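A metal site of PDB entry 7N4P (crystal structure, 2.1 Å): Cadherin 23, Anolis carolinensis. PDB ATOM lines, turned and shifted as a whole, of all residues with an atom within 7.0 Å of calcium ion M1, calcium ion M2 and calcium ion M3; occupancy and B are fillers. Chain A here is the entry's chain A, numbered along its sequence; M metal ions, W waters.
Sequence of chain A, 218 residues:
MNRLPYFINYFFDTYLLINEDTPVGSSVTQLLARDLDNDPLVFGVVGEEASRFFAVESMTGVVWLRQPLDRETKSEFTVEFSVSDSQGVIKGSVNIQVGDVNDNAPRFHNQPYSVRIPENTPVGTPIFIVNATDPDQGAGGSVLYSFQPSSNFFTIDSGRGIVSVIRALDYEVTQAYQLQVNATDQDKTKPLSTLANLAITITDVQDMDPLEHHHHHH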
ATOM      1  N   GLU A  20     -17.814 -23.246  -8.829  1.00  0.00           N
ATOM      2  CA  GLU A  20     -16.990 -23.815  -7.754  1.00  0.00           C
ATOM      3  C   GLU A  20     -17.479 -23.404  -6.349  1.00  0.00           C
ATOM      4  O   GLU A  20     -17.025 -24.049  -5.437  1.00  0.00           O
ATOM      5  CB  GLU A  20     -15.531 -23.402  -7.918  1.00  0.00           C
ATOM      6  CG  GLU A  20     -15.280 -21.943  -7.658  1.00  0.00           C
ATOM      7  CD  GLU A  20     -13.791 -21.622  -7.773  1.00  0.00           C
ATOM      8  OE1 GLU A  20     -12.963 -22.454  -7.301  1.00  0.00           O
ATOM      9  OE2 GLU A  20     -13.472 -20.545  -8.349  1.00  0.00           O
ATOM     10  N   LEU A  69     -16.040 -28.270  -4.679  1.00  0.00           N
ATOM     11  CA  LEU A  69     -15.336 -28.056  -5.958  1.00  0.00           C
ATOM     12  C   LEU A  69     -14.295 -26.948  -5.770  1.00  0.00           C
ATOM     13  O   LEU A  69     -14.413 -26.133  -4.851  1.00  0.00           O
ATOM     14  CB  LEU A  69     -16.384 -27.660  -7.001  1.00  0.00           C
ATOM     15  CG  LEU A  69     -17.454 -28.715  -7.268  1.00  0.00           C
ATOM     16  CD1 LEU A  69     -18.536 -28.135  -8.174  1.00  0.00           C
ATOM     17  CD2 LEU A  69     -16.849 -29.940  -7.886  1.00  0.00           C
ATOM     18  N   ASP A  70     -13.305 -26.931  -6.633  1.00  0.00           N
ATOM     19  CA  ASP A  70     -12.262 -25.865  -6.621  1.00  0.00           C
ATOM     20  C   ASP A  70     -11.725 -25.781  -8.050  1.00  0.00           C
ATOM     21  O   ASP A  70     -10.914 -26.665  -8.442  1.00  0.00           O
ATOM     22  CB  ASP A  70     -11.153 -26.167  -5.633  1.00  0.00           C
ATOM     23  CG  ASP A  70     -10.045 -25.130  -5.687  1.00  0.00           C
ATOM     24  OD1 ASP A  70     -10.219 -24.057  -6.312  1.00  0.00           O
ATOM     25  OD2 ASP A  70      -9.031 -25.409  -5.107  1.00  0.00           O
ATOM     26  N   ARG A  71     -12.209 -24.810  -8.801  1.00  0.00           N
ATOM     27  CA  ARG A  71     -11.755 -24.665 -10.189  1.00  0.00           C
ATOM     28  C   ARG A  71     -10.233 -24.597 -10.256  1.00  0.00           C
ATOM     29  O   ARG A  71      -9.740 -24.973 -11.267  1.00  0.00           O
ATOM     30  CB  ARG A  71     -12.303 -23.402 -10.841  1.00  0.00           C
ATOM     31  CG  ARG A  71     -12.022 -23.382 -12.329  1.00  0.00           C
ATOM     32  CD  ARG A  71     -11.900 -21.981 -12.871  1.00  0.00           C
ATOM     33  NE  ARG A  71     -10.814 -21.195 -12.312  1.00  0.00           N
ATOM     34  CZ  ARG A  71      -9.678 -20.863 -12.936  1.00  0.00           C
ATOM     35  NH1 ARG A  71      -9.424 -21.327 -14.136  1.00  0.00           N
ATOM     36  NH2 ARG A  71      -8.791 -20.097 -12.337  1.00  0.00           N
ATOM     37  N   GLU A  72      -9.526 -24.135  -9.212  1.00  0.00           N
ATOM     38  CA  GLU A  72      -8.075 -23.874  -9.307  1.00  0.00           C
ATOM     39  C   GLU A  72      -7.340 -25.194  -9.082  1.00  0.00           C
ATOM     40  O   GLU A  72      -6.148 -25.263  -9.343  1.00  0.00           O
ATOM     41  CB  GLU A  72      -7.576 -22.838  -8.302  1.00  0.00           C
ATOM     42  CG  GLU A  72      -7.837 -21.417  -8.761  1.00  0.00           C
ATOM     43  CD  GLU A  72      -9.265 -20.894  -8.631  1.00  0.00           C
ATOM     44  OE1 GLU A  72      -9.961 -21.207  -7.672  1.00  0.00           O
ATOM     45  OE2 GLU A  72      -9.665 -20.137  -9.528  1.00  0.00           O
ATOM     46  N   THR A  73      -8.026 -26.207  -8.594  1.00  0.00           N
ATOM     47  CA  THR A  73      -7.380 -27.535  -8.486  1.00  0.00           C
ATOM     48  C   THR A  73      -7.892 -28.374  -9.647  1.00  0.00           C
ATOM     49  O   THR A  73      -7.098 -29.004 -10.280  1.00  0.00           O
ATOM     50  CB  THR A  73      -7.704 -28.187  -7.141  1.00  0.00           C
ATOM     51  OG1 THR A  73      -7.695 -27.151  -6.164  1.00  0.00           O
ATOM     52  CG2 THR A  73      -6.711 -29.268  -6.782  1.00  0.00           C
ATOM     53  N   GLY A  99     -17.189 -23.989 -12.883  1.00  0.00           N
ATOM     54  CA  GLY A  99     -17.150 -22.533 -13.137  1.00  0.00           C
ATOM     55  C   GLY A  99     -16.281 -21.794 -12.129  1.00  0.00           C
ATOM     56  O   GLY A  99     -16.346 -22.123 -10.877  1.00  0.00           O
ATOM     57  N   ASP A 100     -15.506 -20.816 -12.615  1.00  0.00           N
ATOM     58  CA  ASP A 100     -14.682 -19.956 -11.722  1.00  0.00           C
ATOM     59  C   ASP A 100     -15.570 -19.004 -10.915  1.00  0.00           C
ATOM     60  O   ASP A 100     -16.482 -18.402 -11.526  1.00  0.00           O
ATOM     61  CB  ASP A 100     -13.639 -19.149 -12.490  1.00  0.00           C
ATOM     62  CG  ASP A 100     -12.747 -18.376 -11.517  1.00  0.00           C
ATOM     63  OD1 ASP A 100     -11.970 -18.985 -10.766  1.00  0.00           O
ATOM     64  OD2 ASP A 100     -12.900 -17.177 -11.494  1.00  0.00           O
ATOM     65  N   VAL A 101     -15.292 -18.831  -9.616  1.00  0.00           N
ATOM     66  CA  VAL A 101     -15.709 -17.636  -8.856  1.00  0.00           C
ATOM     67  C   VAL A 101     -14.427 -16.924  -8.442  1.00  0.00           C
ATOM     68  O   VAL A 101     -13.312 -17.568  -8.450  1.00  0.00           O
ATOM     69  CB  VAL A 101     -16.557 -18.005  -7.617  1.00  0.00           C
ATOM     70  CG1 VAL A 101     -15.722 -18.205  -6.370  1.00  0.00           C
ATOM     71  CG2 VAL A 101     -17.605 -16.935  -7.328  1.00  0.00           C
ATOM     72  N   ASN A 102     -14.541 -15.633  -8.117  1.00  0.00           N
ATOM     73  CA  ASN A 102     -13.404 -14.853  -7.586  1.00  0.00           C
ATOM     74  C   ASN A 102     -13.228 -15.225  -6.124  1.00  0.00           C
ATOM     75  O   ASN A 102     -13.838 -14.569  -5.298  1.00  0.00           O
ATOM     76  CB  ASN A 102     -13.580 -13.341  -7.721  1.00  0.00           C
ATOM     77  CG  ASN A 102     -12.309 -12.604  -7.330  1.00  0.00           C
ATOM     78  OD1 ASN A 102     -11.206 -13.051  -7.640  1.00  0.00           O
ATOM     79  ND2 ASN A 102     -12.479 -11.479  -6.681  1.00  0.00           N
ATOM     80  N   ASP A 103     -12.404 -16.212  -5.821  1.00  0.00           N
ATOM     81  CA  ASP A 103     -12.287 -16.763  -4.449  1.00  0.00           C
ATOM     82  C   ASP A 103     -10.847 -16.676  -3.948  1.00  0.00           C
ATOM     83  O   ASP A 103     -10.592 -17.308  -2.954  1.00  0.00           O
ATOM     84  CB  ASP A 103     -12.899 -18.176  -4.359  1.00  0.00           C
ATOM     85  CG  ASP A 103     -12.339 -19.263  -5.277  1.00  0.00           C
ATOM     86  OD1 ASP A 103     -11.686 -18.935  -6.258  1.00  0.00           O
ATOM     87  OD2 ASP A 103     -12.611 -20.460  -5.010  1.00  0.00           O
ATOM     88  N   ASN A 104      -9.915 -15.979  -4.622  1.00  0.00           N
ATOM     89  CA  ASN A 104      -8.493 -15.850  -4.166  1.00  0.00           C
ATOM     90  C   ASN A 104      -8.143 -14.357  -4.170  1.00  0.00           C
ATOM     91  O   ASN A 104      -8.394 -13.711  -5.173  1.00  0.00           O
ATOM     92  CB  ASN A 104      -7.501 -16.577  -5.078  1.00  0.00           C
ATOM     93  CG  ASN A 104      -7.715 -18.071  -5.058  1.00  0.00           C
ATOM     94  OD1 ASN A 104      -7.085 -18.752  -4.275  1.00  0.00           O
ATOM     95  ND2 ASN A 104      -8.723 -18.560  -5.769  1.00  0.00           N
ATOM     96  N   ALA A 105      -7.672 -13.847  -3.044  1.00  0.00           N
ATOM     97  CA  ALA A 105      -6.999 -12.536  -2.902  1.00  0.00           C
ATOM     98  C   ALA A 105      -5.628 -12.657  -3.529  1.00  0.00           C
ATOM     99  O   ALA A 105      -5.070 -13.746  -3.608  1.00  0.00           O
ATOM    100  CB  ALA A 105      -6.861 -12.148  -1.442  1.00  0.00           C
ATOM    101  N   PRO A 106      -5.073 -11.528  -4.041  1.00  0.00           N
ATOM    102  CA  PRO A 106      -3.713 -11.544  -4.587  1.00  0.00           C
ATOM    103  C   PRO A 106      -2.688 -12.056  -3.561  1.00  0.00           C
ATOM    104  O   PRO A 106      -2.888 -11.838  -2.360  1.00  0.00           O
ATOM    105  CB  PRO A 106      -3.520 -10.082  -4.996  1.00  0.00           C
ATOM    106  CG  PRO A 106      -4.919  -9.578  -5.294  1.00  0.00           C
ATOM    107  CD  PRO A 106      -5.763 -10.231  -4.223  1.00  0.00           C
ATOM    108  N   ASP A 134      -2.474 -13.859  -8.825  1.00  0.00           N
ATOM    109  CA  ASP A 134      -3.902 -14.114  -8.507  1.00  0.00           C
ATOM    110  C   ASP A 134      -4.360 -15.157  -9.500  1.00  0.00           C
ATOM    111  O   ASP A 134      -4.333 -14.895 -10.712  1.00  0.00           O
ATOM    112  CB  ASP A 134      -4.725 -12.825  -8.559  1.00  0.00           C
ATOM    113  CG  ASP A 134      -6.125 -12.969  -7.994  1.00  0.00           C
ATOM    114  OD1 ASP A 134      -6.783 -13.955  -8.367  1.00  0.00           O
ATOM    115  OD2 ASP A 134      -6.555 -12.099  -7.147  1.00  0.00           O
ATOM    116  N   PRO A 135      -4.775 -16.342  -9.024  1.00  0.00           N
ATOM    117  CA  PRO A 135      -5.069 -17.482  -9.892  1.00  0.00           C
ATOM    118  C   PRO A 135      -6.491 -17.560 -10.481  1.00  0.00           C
ATOM    119  O   PRO A 135      -6.752 -18.463 -11.317  1.00  0.00           O
ATOM    120  CB  PRO A 135      -4.829 -18.619  -8.918  1.00  0.00           C
ATOM    121  CG  PRO A 135      -5.400 -18.097  -7.605  1.00  0.00           C
ATOM    122  CD  PRO A 135      -4.997 -16.649  -7.585  1.00  0.00           C
ATOM    123  N   ASP A 136      -7.366 -16.623 -10.095  1.00  0.00           N
ATOM    124  CA  ASP A 136      -8.786 -16.566 -10.548  1.00  0.00           C
ATOM    125  C   ASP A 136      -8.831 -16.220 -12.048  1.00  0.00           C
ATOM    126  O   ASP A 136      -7.904 -15.634 -12.497  1.00  0.00           O
ATOM    127  CB  ASP A 136      -9.596 -15.608  -9.668  1.00  0.00           C
ATOM    128  CG  ASP A 136      -9.761 -16.111  -8.237  1.00  0.00           C
ATOM    129  OD1 ASP A 136     -10.095 -17.329  -8.060  1.00  0.00           O
ATOM    130  OD2 ASP A 136      -9.494 -15.299  -7.318  1.00  0.00           O
ATOM    131  N   GLN A 137      -9.920 -16.612 -12.727  1.00  0.00           N
ATOM    132  CA  GLN A 137     -10.202 -16.354 -14.146  1.00  0.00           C
ATOM    133  C   GLN A 137     -10.527 -14.877 -14.384  1.00  0.00           C
ATOM    134  O   GLN A 137     -11.072 -14.250 -13.488  1.00  0.00           O
ATOM    135  CB  GLN A 137     -11.356 -17.237 -14.569  1.00  0.00           C
ATOM    136  CG  GLN A 137     -10.957 -18.054 -15.765  1.00  0.00           C
ATOM    137  CD  GLN A 137     -12.027 -19.046 -16.156  1.00  0.00           C
ATOM    138  OE1 GLN A 137     -13.195 -18.898 -15.826  1.00  0.00           O
ATOM    139  NE2 GLN A 137     -11.593 -20.021 -16.920  1.00  0.00           N
ATOM    140  N   ALA A 139     -11.040 -10.841 -14.975  1.00  0.00           N
ATOM    141  CA  ALA A 139     -10.787  -9.611 -14.200  1.00  0.00           C
ATOM    142  C   ALA A 139     -10.413  -9.979 -12.727  1.00  0.00           C
ATOM    143  O   ALA A 139      -9.493  -9.345 -12.173  1.00  0.00           O
ATOM    144  CB  ALA A 139     -12.019  -8.735 -14.294  1.00  0.00           C
ATOM    145  N   GLY A 140     -11.065 -11.003 -12.146  1.00  0.00           N
ATOM    146  CA  GLY A 140     -10.765 -11.518 -10.798  1.00  0.00           C
ATOM    147  C   GLY A 140      -9.340 -12.060 -10.680  1.00  0.00           C
ATOM    148  O   GLY A 140      -8.839 -12.202  -9.532  1.00  0.00           O
ATOM    149  N   GLY A 141      -8.666 -12.322 -11.817  1.00  0.00           N
ATOM    150  CA  GLY A 141      -7.257 -12.720 -11.795  1.00  0.00           C
ATOM    151  C   GLY A 141      -6.264 -11.614 -12.127  1.00  0.00           C
ATOM    152  O   GLY A 141      -5.048 -11.932 -12.219  1.00  0.00           O
ATOM    153  N   SER A 142      -6.763 -10.394 -12.383  1.00  0.00           N
ATOM    154  CA  SER A 142      -5.965  -9.189 -12.777  1.00  0.00           C
ATOM    155  C   SER A 142      -5.806  -8.267 -11.575  1.00  0.00           C
ATOM    156  O   SER A 142      -6.796  -7.926 -10.978  1.00  0.00           O
ATOM    157  CB  SER A 142      -6.569  -8.407 -13.925  1.00  0.00           C
ATOM    158  OG  SER A 142      -6.540  -9.180 -15.096  1.00  0.00           O
ATOM    159  N   ASP A 185      -7.627  -7.267  -6.876  1.00  0.00           N
ATOM    160  CA  ASP A 185      -8.084  -7.843  -8.154  1.00  0.00           C
ATOM    161  C   ASP A 185      -9.189  -6.953  -8.742  1.00  0.00           C
ATOM    162  O   ASP A 185      -9.702  -6.055  -8.042  1.00  0.00           O
ATOM    163  CB  ASP A 185      -8.363  -9.348  -8.007  1.00  0.00           C
ATOM    164  CG  ASP A 185      -9.619  -9.753  -7.261  1.00  0.00           C
ATOM    165  OD1 ASP A 185     -10.591  -8.994  -7.297  1.00  0.00           O
ATOM    166  OD2 ASP A 185      -9.606 -10.858  -6.752  1.00  0.00           O
ATOM    167  N   GLN A 186      -9.513  -7.178 -10.012  1.00  0.00           N
ATOM    168  CA  GLN A 186     -10.404  -6.297 -10.800  1.00  0.00           C
ATOM    169  C   GLN A 186     -11.788  -6.955 -10.993  1.00  0.00           C
ATOM    170  O   GLN A 186     -12.433  -6.599 -11.959  1.00  0.00           O
ATOM    171  CB  GLN A 186      -9.717  -5.956 -12.124  1.00  0.00           C
ATOM    172  CG  GLN A 186      -8.343  -5.318 -11.935  1.00  0.00           C
ATOM    173  CD  GLN A 186      -7.881  -4.699 -13.233  1.00  0.00           C
ATOM    174  OE1 GLN A 186      -6.794  -4.968 -13.731  1.00  0.00           O
ATOM    175  NE2 GLN A 186      -8.749  -3.890 -13.820  1.00  0.00           N
ATOM    176  N   ASP A 187     -12.207  -7.847 -10.089  1.00  0.00           N
ATOM    177  CA  ASP A 187     -13.595  -8.394 -10.054  1.00  0.00           C
ATOM    178  C   ASP A 187     -14.560  -7.208  -9.917  1.00  0.00           C
ATOM    179  O   ASP A 187     -14.366  -6.385  -8.997  1.00  0.00           O
ATOM    180  CB  ASP A 187     -13.824  -9.381  -8.894  1.00  0.00           C
ATOM    181  CG  ASP A 187     -15.164 -10.118  -8.940  1.00  0.00           C
ATOM    182  OD1 ASP A 187     -15.241 -11.090  -9.706  1.00  0.00           O
ATOM    183  OD2 ASP A 187     -16.127  -9.692  -8.252  1.00  0.00           O
ATOM    184  N   LYS A 190     -17.115  -8.341  -6.308  1.00  0.00           N
ATOM    185  CA  LYS A 190     -16.421  -8.565  -4.995  1.00  0.00           C
ATOM    186  C   LYS A 190     -14.906  -8.483  -5.167  1.00  0.00           C
ATOM    187  O   LYS A 190     -14.225  -9.499  -5.099  1.00  0.00           O
ATOM    188  CB  LYS A 190     -16.851  -9.907  -4.369  1.00  0.00           C
ATOM    189  CG  LYS A 190     -16.074 -11.138  -4.857  1.00  0.00           C
ATOM    190  CD  LYS A 190     -16.621 -12.488  -4.386  1.00  0.00           C
ATOM    191  CE  LYS A 190     -18.033 -12.833  -4.852  1.00  0.00           C
ATOM    192  NZ  LYS A 190     -18.456 -14.188  -4.400  1.00  0.00           N
ATOM    193  N   PRO A 191     -14.293  -7.300  -5.384  1.00  0.00           N
ATOM    194  CA  PRO A 191     -12.860  -7.278  -5.651  1.00  0.00           C
ATOM    195  C   PRO A 191     -12.188  -7.742  -4.357  1.00  0.00           C
ATOM    196  O   PRO A 191     -12.717  -7.403  -3.346  1.00  0.00           O
ATOM    197  CB  PRO A 191     -12.557  -5.819  -5.948  1.00  0.00           C
ATOM    198  CG  PRO A 191     -13.652  -5.082  -5.198  1.00  0.00           C
ATOM    199  CD  PRO A 191     -14.879  -5.962  -5.320  1.00  0.00           C
ATOM    200  N   LEU A 192     -11.130  -8.554  -4.403  1.00  0.00           N
ATOM    201  CA  LEU A 192     -10.387  -8.959  -3.193  1.00  0.00           C
ATOM    202  C   LEU A 192      -9.019  -8.288  -3.212  1.00  0.00           C
ATOM    203  O   LEU A 192      -8.495  -8.047  -4.322  1.00  0.00           O
ATOM    204  CB  LEU A 192     -10.268 -10.479  -3.157  1.00  0.00           C
ATOM    205  CG  LEU A 192     -11.617 -11.208  -3.195  1.00  0.00           C
ATOM    206  CD1 LEU A 192     -11.429 -12.712  -3.130  1.00  0.00           C
ATOM    207  CD2 LEU A 192     -12.535 -10.727  -2.080  1.00  0.00           C
HETATM  208 CA    CA M   1     -11.204 -22.006  -5.923  1.00  0.00          CA
HETATM  209 CA    CA M   2     -11.545 -19.151  -8.542  1.00  0.00          CA
HETATM  210 CA    CA M   3      -8.899 -13.007  -7.300  1.00  0.00          CA
HETATM  211  O   HOH W   1      -9.415 -21.357  -4.638  1.00  0.00           O
HETATM  212  O   HOH W   2     -12.002 -23.026  -4.181  1.00  0.00           O
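The side-chain carboxylate (OE1) of Glu 20 lies close to the backbone NH (N) of Arg 71.
The side-chain carboxylate (OD2) of Asp 100 lies within hydrogen-bond range of the backbone NH (N) of Gln 137 (3.3 Å).
The backbone carbonyl oxygen of Lys 190 is in hydrogen-bond range of the side-chain amide nitrogen of Asn 102 (3.1 Å).
The backbone carbonyl oxygen of Asp 136 lies close to the backbone NH of Gly 141, 3.5 Å away.
OD1 of Asp 100 lies close to NE of Arg 71 (2.9 Å).
OE1 of Glu 72 lies close to ND2 of Asn 104 (3.5 Å).
OD1 of Asp 185 sits close to N of Asp 187 (3.4 Å).
O of Gly 99 sits at hydrogen-bond distance from N of Glu 20 (2.8 Å).
Four residues have an atom within 4 Å of calcium ion M1: Glu 20, Asp 70, Glu 72 and Asp 103.
Six residues have an atom within 4 Å of calcium ion M2: Glu 20, Glu 72, Asp 100, Val 101, Asp 103 and Asp 136.
Along chain A the residues within 4 Å of calcium ion M2 span positions 20 to 136.
The nearest printed residue that does not touch calcium ion M2 is Asn 104 (4.0003 Å).
Six residues have an atom within 4 Å of calcium ion M3: Asn 102, Asn 104, Asp 134, Asp 136, Gly 140 and Asp 185.
Along chain A the residues within 4 Å of calcium ion M3 span positions 102 to 185.
The nearest printed residue that does not touch calcium ion M3 is Ala 105 (4.5 Å).
Water W2 is bound to calcium ion M1 (2.2 Å).
Calcium ion M1 is bound by OE1 of Glu 20 (2.3 Å).
Calcium ion M1 is bound by the side-chain carboxylate (OD2) of Asp 103, 2.3 Å away.
OE1 of Glu 72 binds calcium ion M1.
Water W1 is bound to calcium ion M1 (2.3 Å).
OD1 of Asp 70 binds calcium ion M1 (2.3 Å).
Slightly farther from calcium ion M1 lies the side-chain carboxylate (OD1) of Asp 103 (3.1 Å).
Calcium ion M2 is bound by OD1 of Asp 100, OD1 of Asp 103, OE2 of Glu 72, O of Val 101, OD1 of Asp 136, OE2 of Glu 20 and OE1 of Glu 72.
Calcium ion M3 is bound by O of Asn 104 (2.3 Å).
The side-chain carboxylate (OD2) of Asp 185 binds calcium ion M3 (2.3 Å).
The side-chain amide oxygen (OD1) of Asn 102 is bound to calcium ion M3 (2.3 Å).
OD2 of Asp 136 binds calcium ion M3, 2.4 Å away.
O of Gly 140 binds calcium ion M3 (2.4 Å).
Calcium ion M3 is bound by the side-chain carboxylate (OD2) of Asp 134 (2.5 Å).
The side-chain carboxylate (OD1) of Asp 134 binds calcium ion M3.
Calcium ion M3 has seven donor atoms within binding distance.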
